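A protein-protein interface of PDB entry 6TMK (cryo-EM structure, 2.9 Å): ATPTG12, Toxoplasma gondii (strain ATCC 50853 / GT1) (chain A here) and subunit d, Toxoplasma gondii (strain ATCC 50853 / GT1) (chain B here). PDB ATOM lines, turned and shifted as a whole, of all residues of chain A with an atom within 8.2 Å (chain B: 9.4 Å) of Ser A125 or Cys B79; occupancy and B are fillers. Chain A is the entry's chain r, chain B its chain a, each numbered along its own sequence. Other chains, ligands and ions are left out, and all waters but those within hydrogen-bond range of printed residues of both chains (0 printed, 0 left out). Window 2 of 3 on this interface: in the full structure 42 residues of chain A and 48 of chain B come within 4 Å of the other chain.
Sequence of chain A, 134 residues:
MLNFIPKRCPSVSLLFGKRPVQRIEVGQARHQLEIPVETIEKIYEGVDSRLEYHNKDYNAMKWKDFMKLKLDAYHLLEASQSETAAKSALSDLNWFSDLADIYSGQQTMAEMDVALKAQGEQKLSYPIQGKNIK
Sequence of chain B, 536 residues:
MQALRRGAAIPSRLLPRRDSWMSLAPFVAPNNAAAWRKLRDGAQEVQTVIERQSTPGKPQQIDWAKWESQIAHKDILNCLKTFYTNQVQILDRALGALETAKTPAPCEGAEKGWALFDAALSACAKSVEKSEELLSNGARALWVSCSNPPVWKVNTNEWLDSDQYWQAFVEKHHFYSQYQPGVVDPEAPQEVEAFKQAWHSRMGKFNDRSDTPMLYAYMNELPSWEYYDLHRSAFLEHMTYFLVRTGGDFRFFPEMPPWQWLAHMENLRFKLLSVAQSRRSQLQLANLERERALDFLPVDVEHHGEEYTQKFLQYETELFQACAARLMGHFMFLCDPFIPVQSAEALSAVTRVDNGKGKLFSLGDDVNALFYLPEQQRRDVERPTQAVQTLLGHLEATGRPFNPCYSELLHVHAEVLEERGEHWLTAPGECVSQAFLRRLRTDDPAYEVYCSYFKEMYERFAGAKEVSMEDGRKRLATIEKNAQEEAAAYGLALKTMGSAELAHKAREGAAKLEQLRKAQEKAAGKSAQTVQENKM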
ATOM      1  N   GLU A 121     -26.074 -25.445 -22.862  1.00  0.00           N
ATOM      2  CA  GLU A 121     -24.926 -24.797 -23.488  1.00  0.00           C
ATOM      3  C   GLU A 121     -25.146 -23.282 -23.563  1.00  0.00           C
ATOM      4  O   GLU A 121     -25.314 -22.674 -24.623  1.00  0.00           O
ATOM      5  CB  GLU A 121     -24.664 -25.384 -24.882  1.00  0.00           C
ATOM      6  CG  GLU A 121     -23.939 -26.718 -24.867  1.00  0.00           C
ATOM      7  CD  GLU A 121     -22.435 -26.561 -24.750  1.00  0.00           C
ATOM      8  OE1 GLU A 121     -21.985 -25.585 -24.113  1.00  0.00           O
ATOM      9  OE2 GLU A 121     -21.702 -27.413 -25.295  1.00  0.00           O
ATOM     10  N   GLN A 122     -25.139 -22.704 -22.361  1.00  0.00           N
ATOM     11  CA  GLN A 122     -25.269 -21.261 -22.191  1.00  0.00           C
ATOM     12  C   GLN A 122     -24.192 -20.533 -22.983  1.00  0.00           C
ATOM     13  O   GLN A 122     -24.485 -19.788 -23.925  1.00  0.00           O
ATOM     14  CB  GLN A 122     -25.198 -20.914 -20.702  1.00  0.00           C
ATOM     15  CG  GLN A 122     -25.130 -19.423 -20.397  1.00  0.00           C
ATOM     16  CD  GLN A 122     -23.714 -18.932 -20.152  1.00  0.00           C
ATOM     17  OE1 GLN A 122     -22.779 -19.723 -20.038  1.00  0.00           O
ATOM     18  NE2 GLN A 122     -23.553 -17.617 -20.067  1.00  0.00           N
ATOM     19  N   LYS A 123     -22.932 -20.741 -22.613  1.00  0.00           N
ATOM     20  CA  LYS A 123     -21.812 -20.163 -23.339  1.00  0.00           C
ATOM     21  C   LYS A 123     -20.606 -21.058 -23.104  1.00  0.00           C
ATOM     22  O   LYS A 123     -20.600 -21.902 -22.203  1.00  0.00           O
ATOM     23  CB  LYS A 123     -21.521 -18.733 -22.860  1.00  0.00           C
ATOM     24  CG  LYS A 123     -22.432 -17.627 -23.409  1.00  0.00           C
ATOM     25  CD  LYS A 123     -22.561 -17.583 -24.927  1.00  0.00           C
ATOM     26  CE  LYS A 123     -21.746 -16.438 -25.497  1.00  0.00           C
ATOM     27  NZ  LYS A 123     -21.752 -16.425 -26.983  1.00  0.00           N
ATOM     28  N   LEU A 124     -19.576 -20.872 -23.926  1.00  0.00           N
ATOM     29  CA  LEU A 124     -18.338 -21.627 -23.795  1.00  0.00           C
ATOM     30  C   LEU A 124     -17.152 -20.676 -23.711  1.00  0.00           C
ATOM     31  O   LEU A 124     -17.256 -19.484 -24.013  1.00  0.00           O
ATOM     32  CB  LEU A 124     -18.159 -22.588 -24.979  1.00  0.00           C
ATOM     33  CG  LEU A 124     -18.718 -24.009 -24.854  1.00  0.00           C
ATOM     34  CD1 LEU A 124     -18.269 -24.845 -26.037  1.00  0.00           C
ATOM     35  CD2 LEU A 124     -18.299 -24.675 -23.552  1.00  0.00           C
ATOM     36  N   SER A 125     -16.010 -21.224 -23.291  1.00  0.00           N
ATOM     37  CA  SER A 125     -14.772 -20.461 -23.137  1.00  0.00           C
ATOM     38  C   SER A 125     -13.637 -21.255 -23.781  1.00  0.00           C
ATOM     39  O   SER A 125     -13.009 -22.093 -23.128  1.00  0.00           O
ATOM     40  CB  SER A 125     -14.492 -20.171 -21.666  1.00  0.00           C
ATOM     41  OG  SER A 125     -14.703 -21.322 -20.869  1.00  0.00           O
ATOM     42  N   TYR A 126     -13.376 -20.991 -25.059  1.00  0.00           N
ATOM     43  CA  TYR A 126     -12.299 -21.670 -25.776  1.00  0.00           C
ATOM     44  C   TYR A 126     -11.029 -20.832 -25.713  1.00  0.00           C
ATOM     45  O   TYR A 126     -11.057 -19.656 -26.091  1.00  0.00           O
ATOM     46  CB  TYR A 126     -12.671 -21.912 -27.231  1.00  0.00           C
ATOM     47  CG  TYR A 126     -13.471 -23.170 -27.469  1.00  0.00           C
ATOM     48  CD1 TYR A 126     -12.848 -24.411 -27.507  1.00  0.00           C
ATOM     49  CD2 TYR A 126     -14.842 -23.120 -27.671  1.00  0.00           C
ATOM     50  CE1 TYR A 126     -13.570 -25.566 -27.728  1.00  0.00           C
ATOM     51  CE2 TYR A 126     -15.573 -24.270 -27.898  1.00  0.00           C
ATOM     52  CZ  TYR A 126     -14.932 -25.490 -27.922  1.00  0.00           C
ATOM     53  OH  TYR A 126     -15.656 -26.639 -28.144  1.00  0.00           O
ATOM     54  N   PRO A 127      -9.899 -21.374 -25.252  1.00  0.00           N
ATOM     55  CA  PRO A 127      -8.648 -20.612 -25.346  1.00  0.00           C
ATOM     56  C   PRO A 127      -8.140 -20.614 -26.780  1.00  0.00           C
ATOM     57  O   PRO A 127      -7.954 -21.672 -27.386  1.00  0.00           O
ATOM     58  CB  PRO A 127      -7.699 -21.369 -24.409  1.00  0.00           C
ATOM     59  CG  PRO A 127      -8.200 -22.769 -24.446  1.00  0.00           C
ATOM     60  CD  PRO A 127      -9.701 -22.663 -24.562  1.00  0.00           C
ATOM     61  N   ILE A 128      -7.917 -19.418 -27.319  1.00  0.00           N
ATOM     62  CA  ILE A 128      -7.529 -19.242 -28.713  1.00  0.00           C
ATOM     63  C   ILE A 128      -6.257 -18.411 -28.768  1.00  0.00           C
ATOM     64  O   ILE A 128      -6.128 -17.406 -28.060  1.00  0.00           O
ATOM     65  CB  ILE A 128      -8.650 -18.574 -29.535  1.00  0.00           C
ATOM     66  CG1 ILE A 128      -9.280 -17.429 -28.740  1.00  0.00           C
ATOM     67  CG2 ILE A 128      -9.703 -19.600 -29.925  1.00  0.00           C
ATOM     68  CD1 ILE A 128     -10.133 -16.504 -29.577  1.00  0.00           C
ATOM     69  N   ASN A 132      -6.921 -15.048 -26.109  1.00  0.00           N
ATOM     70  CA  ASN A 132      -7.000 -15.429 -24.704  1.00  0.00           C
ATOM     71  C   ASN A 132      -5.629 -15.592 -24.062  1.00  0.00           C
ATOM     72  O   ASN A 132      -5.530 -15.555 -22.832  1.00  0.00           O
ATOM     73  CB  ASN A 132      -7.807 -16.720 -24.546  1.00  0.00           C
ATOM     74  CG  ASN A 132      -9.284 -16.516 -24.826  1.00  0.00           C
ATOM     75  OD1 ASN A 132      -9.698 -15.446 -25.272  1.00  0.00           O
ATOM     76  ND2 ASN A 132     -10.091 -17.526 -24.526  1.00  0.00           N
ATOM     77  N   TRP B  64      -9.578 -25.314  -6.877  1.00  0.00           N
ATOM     78  CA  TRP B  64      -8.704 -24.523  -7.734  1.00  0.00           C
ATOM     79  C   TRP B  64      -7.681 -23.714  -6.947  1.00  0.00           C
ATOM     80  O   TRP B  64      -6.745 -23.179  -7.552  1.00  0.00           O
ATOM     81  CB  TRP B  64      -9.545 -23.583  -8.596  1.00  0.00           C
ATOM     82  CG  TRP B  64     -10.617 -24.290  -9.361  1.00  0.00           C
ATOM     83  CD1 TRP B  64     -11.895 -24.524  -8.948  1.00  0.00           C
ATOM     84  CD2 TRP B  64     -10.504 -24.865 -10.666  1.00  0.00           C
ATOM     85  NE1 TRP B  64     -12.588 -25.206  -9.918  1.00  0.00           N
ATOM     86  CE2 TRP B  64     -11.757 -25.427 -10.983  1.00  0.00           C
ATOM     87  CE3 TRP B  64      -9.468 -24.958 -11.599  1.00  0.00           C
ATOM     88  CZ2 TRP B  64     -12.000 -26.072 -12.193  1.00  0.00           C
ATOM     89  CZ3 TRP B  64      -9.710 -25.599 -12.800  1.00  0.00           C
ATOM     90  CH2 TRP B  64     -10.967 -26.149 -13.084  1.00  0.00           C
ATOM     91  N   GLU B  68      -4.209 -22.889  -8.959  1.00  0.00           N
ATOM     92  CA  GLU B  68      -3.860 -21.501  -9.237  1.00  0.00           C
ATOM     93  C   GLU B  68      -2.484 -21.166  -8.685  1.00  0.00           C
ATOM     94  O   GLU B  68      -1.747 -20.375  -9.285  1.00  0.00           O
ATOM     95  CB  GLU B  68      -4.917 -20.566  -8.648  1.00  0.00           C
ATOM     96  CG  GLU B  68      -5.984 -20.143  -9.643  1.00  0.00           C
ATOM     97  CD  GLU B  68      -7.304 -19.813  -8.976  1.00  0.00           C
ATOM     98  OE1 GLU B  68      -7.288 -19.362  -7.811  1.00  0.00           O
ATOM     99  OE2 GLU B  68      -8.360 -20.004  -9.617  1.00  0.00           O
ATOM    100  N   LYS B  74      -1.745 -19.422 -15.581  1.00  0.00           N
ATOM    101  CA  LYS B  74      -2.917 -18.750 -15.021  1.00  0.00           C
ATOM    102  C   LYS B  74      -3.626 -17.884 -16.059  1.00  0.00           C
ATOM    103  O   LYS B  74      -4.187 -16.835 -15.730  1.00  0.00           O
ATOM    104  CB  LYS B  74      -2.535 -17.916 -13.797  1.00  0.00           C
ATOM    105  CG  LYS B  74      -1.668 -18.666 -12.796  1.00  0.00           C
ATOM    106  CD  LYS B  74      -1.433 -17.853 -11.534  1.00  0.00           C
ATOM    107  CE  LYS B  74      -0.389 -16.770 -11.752  1.00  0.00           C
ATOM    108  NZ  LYS B  74       0.996 -17.315 -11.698  1.00  0.00           N
ATOM    109  N   ASP B  75      -3.605 -18.314 -17.316  1.00  0.00           N
ATOM    110  CA  ASP B  75      -4.297 -17.631 -18.403  1.00  0.00           C
ATOM    111  C   ASP B  75      -5.296 -18.533 -19.107  1.00  0.00           C
ATOM    112  O   ASP B  75      -6.371 -18.072 -19.495  1.00  0.00           O
ATOM    113  CB  ASP B  75      -3.282 -17.097 -19.424  1.00  0.00           C
ATOM    114  CG  ASP B  75      -2.260 -18.141 -19.831  1.00  0.00           C
ATOM    115  OD1 ASP B  75      -2.492 -19.338 -19.568  1.00  0.00           O
ATOM    116  OD2 ASP B  75      -1.224 -17.763 -20.419  1.00  0.00           O
ATOM    117  N   ILE B  76      -4.962 -19.809 -19.278  1.00  0.00           N
ATOM    118  CA  ILE B  76      -5.908 -20.781 -19.809  1.00  0.00           C
ATOM    119  C   ILE B  76      -6.609 -21.514 -18.668  1.00  0.00           C
ATOM    120  O   ILE B  76      -7.743 -21.976 -18.832  1.00  0.00           O
ATOM    121  CB  ILE B  76      -5.208 -21.767 -20.761  1.00  0.00           C
ATOM    122  CG1 ILE B  76      -4.363 -22.774 -19.977  1.00  0.00           C
ATOM    123  CG2 ILE B  76      -4.351 -21.007 -21.764  1.00  0.00           C
ATOM    124  CD1 ILE B  76      -3.512 -23.665 -20.854  1.00  0.00           C
ATOM    125  N   LEU B  77      -5.925 -21.676 -17.533  1.00  0.00           N
ATOM    126  CA  LEU B  77      -6.553 -22.243 -16.347  1.00  0.00           C
ATOM    127  C   LEU B  77      -7.837 -21.502 -15.994  1.00  0.00           C
ATOM    128  O   LEU B  77      -8.826 -22.120 -15.585  1.00  0.00           O
ATOM    129  CB  LEU B  77      -5.572 -22.203 -15.173  1.00  0.00           C
ATOM    130  CG  LEU B  77      -6.032 -22.843 -13.863  1.00  0.00           C
ATOM    131  CD1 LEU B  77      -6.150 -24.351 -14.008  1.00  0.00           C
ATOM    132  CD2 LEU B  77      -5.075 -22.486 -12.736  1.00  0.00           C
ATOM    133  N   ASN B  78      -7.845 -20.178 -16.152  1.00  0.00           N
ATOM    134  CA  ASN B  78      -9.024 -19.398 -15.787  1.00  0.00           C
ATOM    135  C   ASN B  78     -10.204 -19.731 -16.693  1.00  0.00           C
ATOM    136  O   ASN B  78     -11.322 -19.958 -16.217  1.00  0.00           O
ATOM    137  CB  ASN B  78      -8.702 -17.906 -15.850  1.00  0.00           C
ATOM    138  CG  ASN B  78      -9.724 -17.059 -15.119  1.00  0.00           C
ATOM    139  OD1 ASN B  78     -10.716 -17.572 -14.600  1.00  0.00           O
ATOM    140  ND2 ASN B  78      -9.486 -15.754 -15.075  1.00  0.00           N
ATOM    141  N   CYS B  79      -9.972 -19.782 -18.007  1.00  0.00           N
ATOM    142  CA  CYS B  79     -11.060 -20.096 -18.927  1.00  0.00           C
ATOM    143  C   CYS B  79     -11.534 -21.529 -18.724  1.00  0.00           C
ATOM    144  O   CYS B  79     -12.735 -21.814 -18.806  1.00  0.00           O
ATOM    145  CB  CYS B  79     -10.627 -19.863 -20.376  1.00  0.00           C
ATOM    146  SG  CYS B  79      -9.735 -21.227 -21.155  1.00  0.00           S
ATOM    147  N   LEU B  80     -10.597 -22.450 -18.495  1.00  0.00           N
ATOM    148  CA  LEU B  80     -10.962 -23.832 -18.207  1.00  0.00           C
ATOM    149  C   LEU B  80     -11.853 -23.923 -16.969  1.00  0.00           C
ATOM    150  O   LEU B  80     -12.878 -24.613 -16.978  1.00  0.00           O
ATOM    151  CB  LEU B  80      -9.689 -24.661 -18.032  1.00  0.00           C
ATOM    152  CG  LEU B  80      -9.814 -26.144 -17.687  1.00  0.00           C
ATOM    153  CD1 LEU B  80      -8.669 -26.914 -18.326  1.00  0.00           C
ATOM    154  CD2 LEU B  80      -9.810 -26.343 -16.182  1.00  0.00           C
ATOM    155  N   LYS B  81     -11.454 -23.258 -15.880  1.00  0.00           N
ATOM    156  CA  LYS B  81     -12.286 -23.232 -14.680  1.00  0.00           C
ATOM    157  C   LYS B  81     -13.653 -22.619 -14.963  1.00  0.00           C
ATOM    158  O   LYS B  81     -14.667 -23.051 -14.399  1.00  0.00           O
ATOM    159  CB  LYS B  81     -11.565 -22.459 -13.576  1.00  0.00           C
ATOM    160  CG  LYS B  81     -12.418 -22.139 -12.360  1.00  0.00           C
ATOM    161  CD  LYS B  81     -11.578 -21.507 -11.263  1.00  0.00           C
ATOM    162  CE  LYS B  81     -12.380 -21.303  -9.990  1.00  0.00           C
ATOM    163  NZ  LYS B  81     -13.291 -20.131 -10.094  1.00  0.00           N
ATOM    164  N   THR B  82     -13.699 -21.597 -15.821  1.00  0.00           N
ATOM    165  CA  THR B  82     -14.979 -20.988 -16.170  1.00  0.00           C
ATOM    166  C   THR B  82     -15.873 -21.998 -16.874  1.00  0.00           C
ATOM    167  O   THR B  82     -17.061 -22.126 -16.562  1.00  0.00           O
ATOM    168  CB  THR B  82     -14.755 -19.759 -17.053  1.00  0.00           C
ATOM    169  OG1 THR B  82     -13.712 -18.947 -16.497  1.00  0.00           O
ATOM    170  CG2 THR B  82     -16.031 -18.939 -17.159  1.00  0.00           C
ATOM    171  N   PHE B  83     -15.301 -22.729 -17.831  1.00  0.00           N
ATOM    172  CA  PHE B  83     -16.020 -23.811 -18.498  1.00  0.00           C
ATOM    173  C   PHE B  83     -16.539 -24.821 -17.482  1.00  0.00           C
ATOM    174  O   PHE B  83     -17.689 -25.271 -17.560  1.00  0.00           O
ATOM    175  CB  PHE B  83     -15.106 -24.483 -19.522  1.00  0.00           C
ATOM    176  CG  PHE B  83     -15.492 -25.895 -19.846  1.00  0.00           C
ATOM    177  CD1 PHE B  83     -16.438 -26.161 -20.822  1.00  0.00           C
ATOM    178  CD2 PHE B  83     -14.893 -26.958 -19.193  1.00  0.00           C
ATOM    179  CE1 PHE B  83     -16.790 -27.459 -21.128  1.00  0.00           C
ATOM    180  CE2 PHE B  83     -15.239 -28.258 -19.495  1.00  0.00           C
ATOM    181  CZ  PHE B  83     -16.191 -28.509 -20.463  1.00  0.00           C
ATOM    182  N   TYR B  84     -15.678 -25.228 -16.549  1.00  0.00           N
ATOM    183  CA  TYR B  84     -16.081 -26.196 -15.534  1.00  0.00           C
ATOM    184  C   TYR B  84     -17.291 -25.705 -14.748  1.00  0.00           C
ATOM    185  O   TYR B  84     -18.287 -26.425 -14.616  1.00  0.00           O
ATOM    186  CB  TYR B  84     -14.915 -26.480 -14.588  1.00  0.00           C
ATOM    187  CG  TYR B  84     -15.267 -27.413 -13.451  1.00  0.00           C
ATOM    188  CD1 TYR B  84     -15.149 -28.788 -13.586  1.00  0.00           C
ATOM    189  CD2 TYR B  84     -15.690 -26.912 -12.227  1.00  0.00           C
ATOM    190  CE1 TYR B  84     -15.462 -29.640 -12.544  1.00  0.00           C
ATOM    191  CE2 TYR B  84     -16.006 -27.754 -11.179  1.00  0.00           C
ATOM    192  CZ  TYR B  84     -15.889 -29.117 -11.342  1.00  0.00           C
ATOM    193  OH  TYR B  84     -16.202 -29.960 -10.301  1.00  0.00           O
ATOM    194  N   THR B  85     -17.204 -24.503 -14.177  1.00  0.00           N
ATOM    195  CA  THR B  85     -18.320 -23.993 -13.385  1.00  0.00           C
ATOM    196  C   THR B  85     -19.548 -23.693 -14.235  1.00  0.00           C
ATOM    197  O   THR B  85     -20.675 -23.843 -13.741  1.00  0.00           O
ATOM    198  CB  THR B  85     -17.897 -22.727 -12.637  1.00  0.00           C
ATOM    199  OG1 THR B  85     -17.490 -21.727 -13.577  1.00  0.00           O
ATOM    200  CG2 THR B  85     -16.747 -23.028 -11.689  1.00  0.00           C
ATOM    201  N   ASN B  86     -19.370 -23.532 -15.546  1.00  0.00           N
ATOM    202  CA  ASN B  86     -20.503 -23.296 -16.431  1.00  0.00           C
ATOM    203  C   ASN B  86     -21.194 -24.597 -16.780  1.00  0.00           C
ATOM    204  O   ASN B  86     -22.403 -24.605 -17.039  1.00  0.00           O
ATOM    205  CB  ASN B  86     -20.038 -22.591 -17.706  1.00  0.00           C
ATOM    206  CG  ASN B  86     -21.166 -21.879 -18.423  1.00  0.00           C
ATOM    207  OD1 ASN B  86     -22.336 -22.021 -18.065  1.00  0.00           O
ATOM    208  ND2 ASN B  86     -20.820 -21.108 -19.446  1.00  0.00           N
ATOM    209  N   GLN B  87     -20.452 -25.697 -16.786  1.00  0.00           N
ATOM    210  CA  GLN B  87     -21.089 -26.969 -17.072  1.00  0.00           C
ATOM    211  C   GLN B  87     -21.705 -27.514 -15.793  1.00  0.00           C
ATOM    212  O   GLN B  87     -22.775 -28.127 -15.828  1.00  0.00           O
ATOM    213  CB  GLN B  87     -20.077 -27.955 -17.653  1.00  0.00           C
ATOM    214  CG  GLN B  87     -19.692 -27.669 -19.093  1.00  0.00           C
ATOM    215  CD  GLN B  87     -20.792 -28.032 -20.070  1.00  0.00           C
ATOM    216  OE1 GLN B  87     -21.405 -29.094 -19.965  1.00  0.00           O
ATOM    217  NE2 GLN B  87     -21.050 -27.149 -21.027  1.00  0.00           N
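The side-chain amide nitrogen (ND2) of Asn B86 sits at hydrogen-bond distance from the side-chain amide oxygen (OE1) of Gln A122 (2.5 Å). The backbone carbonyl oxygen (O) of Lys A123 sits at hydrogen-bond distance from the side-chain amide nitrogen (ND2) of Asn B86, at 2.9 Å. OG of Ser A125 is in hydrogen-bond range of O of Cys B79 (2.9 Å). The backbone NH (N) of Phe B83 sits at hydrogen-bond distance from the side-chain hydroxyl (OG) of Ser A125 (3.4 Å).
O of Ile B76 lies within hydrogen-bond range of SG of Cys B79, at 3.2 Å.
OE1 of Glu A121 touches NE2 of Gln B87, 3.6 Å away. Leu A124 touches Phe B83. Pro A127 touches Cys B79.
Ser A125 touches just these residues of chain B: Cys B79 (2.9 Å) and Phe B83 (3.4 Å). Of chain B, only Phe B83 (3.6 Å) comes within 4 Å of Leu A124. Of the printed residues of chain B, Glu A121 touches Gln B87. Of the printed residues of chain B, Pro A127 touches Cys B79. Of the printed residues of chain A, Phe B83 touches Leu A124 (3.6 Å) and Ser A125 (3.4 Å). Printed residues of chain A within 4 Å of Gln B87: Glu A121 (3.6 Å). The nearest residue of chain B that does not touch Ser A125 is Thr B82 (4.1 Å). The nearest printed residue of chain B that does not touch Lys A123 is Gln B87 (5.4 Å).
Of the 9 printed residues of chain A, 6 touch a printed residue of chain B. Of the 16 printed residues of chain B, 4 touch a printed residue of chain A. Hydrophobic or aromatic side chains of chain B that line the printed part of chain A: Phe B83.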
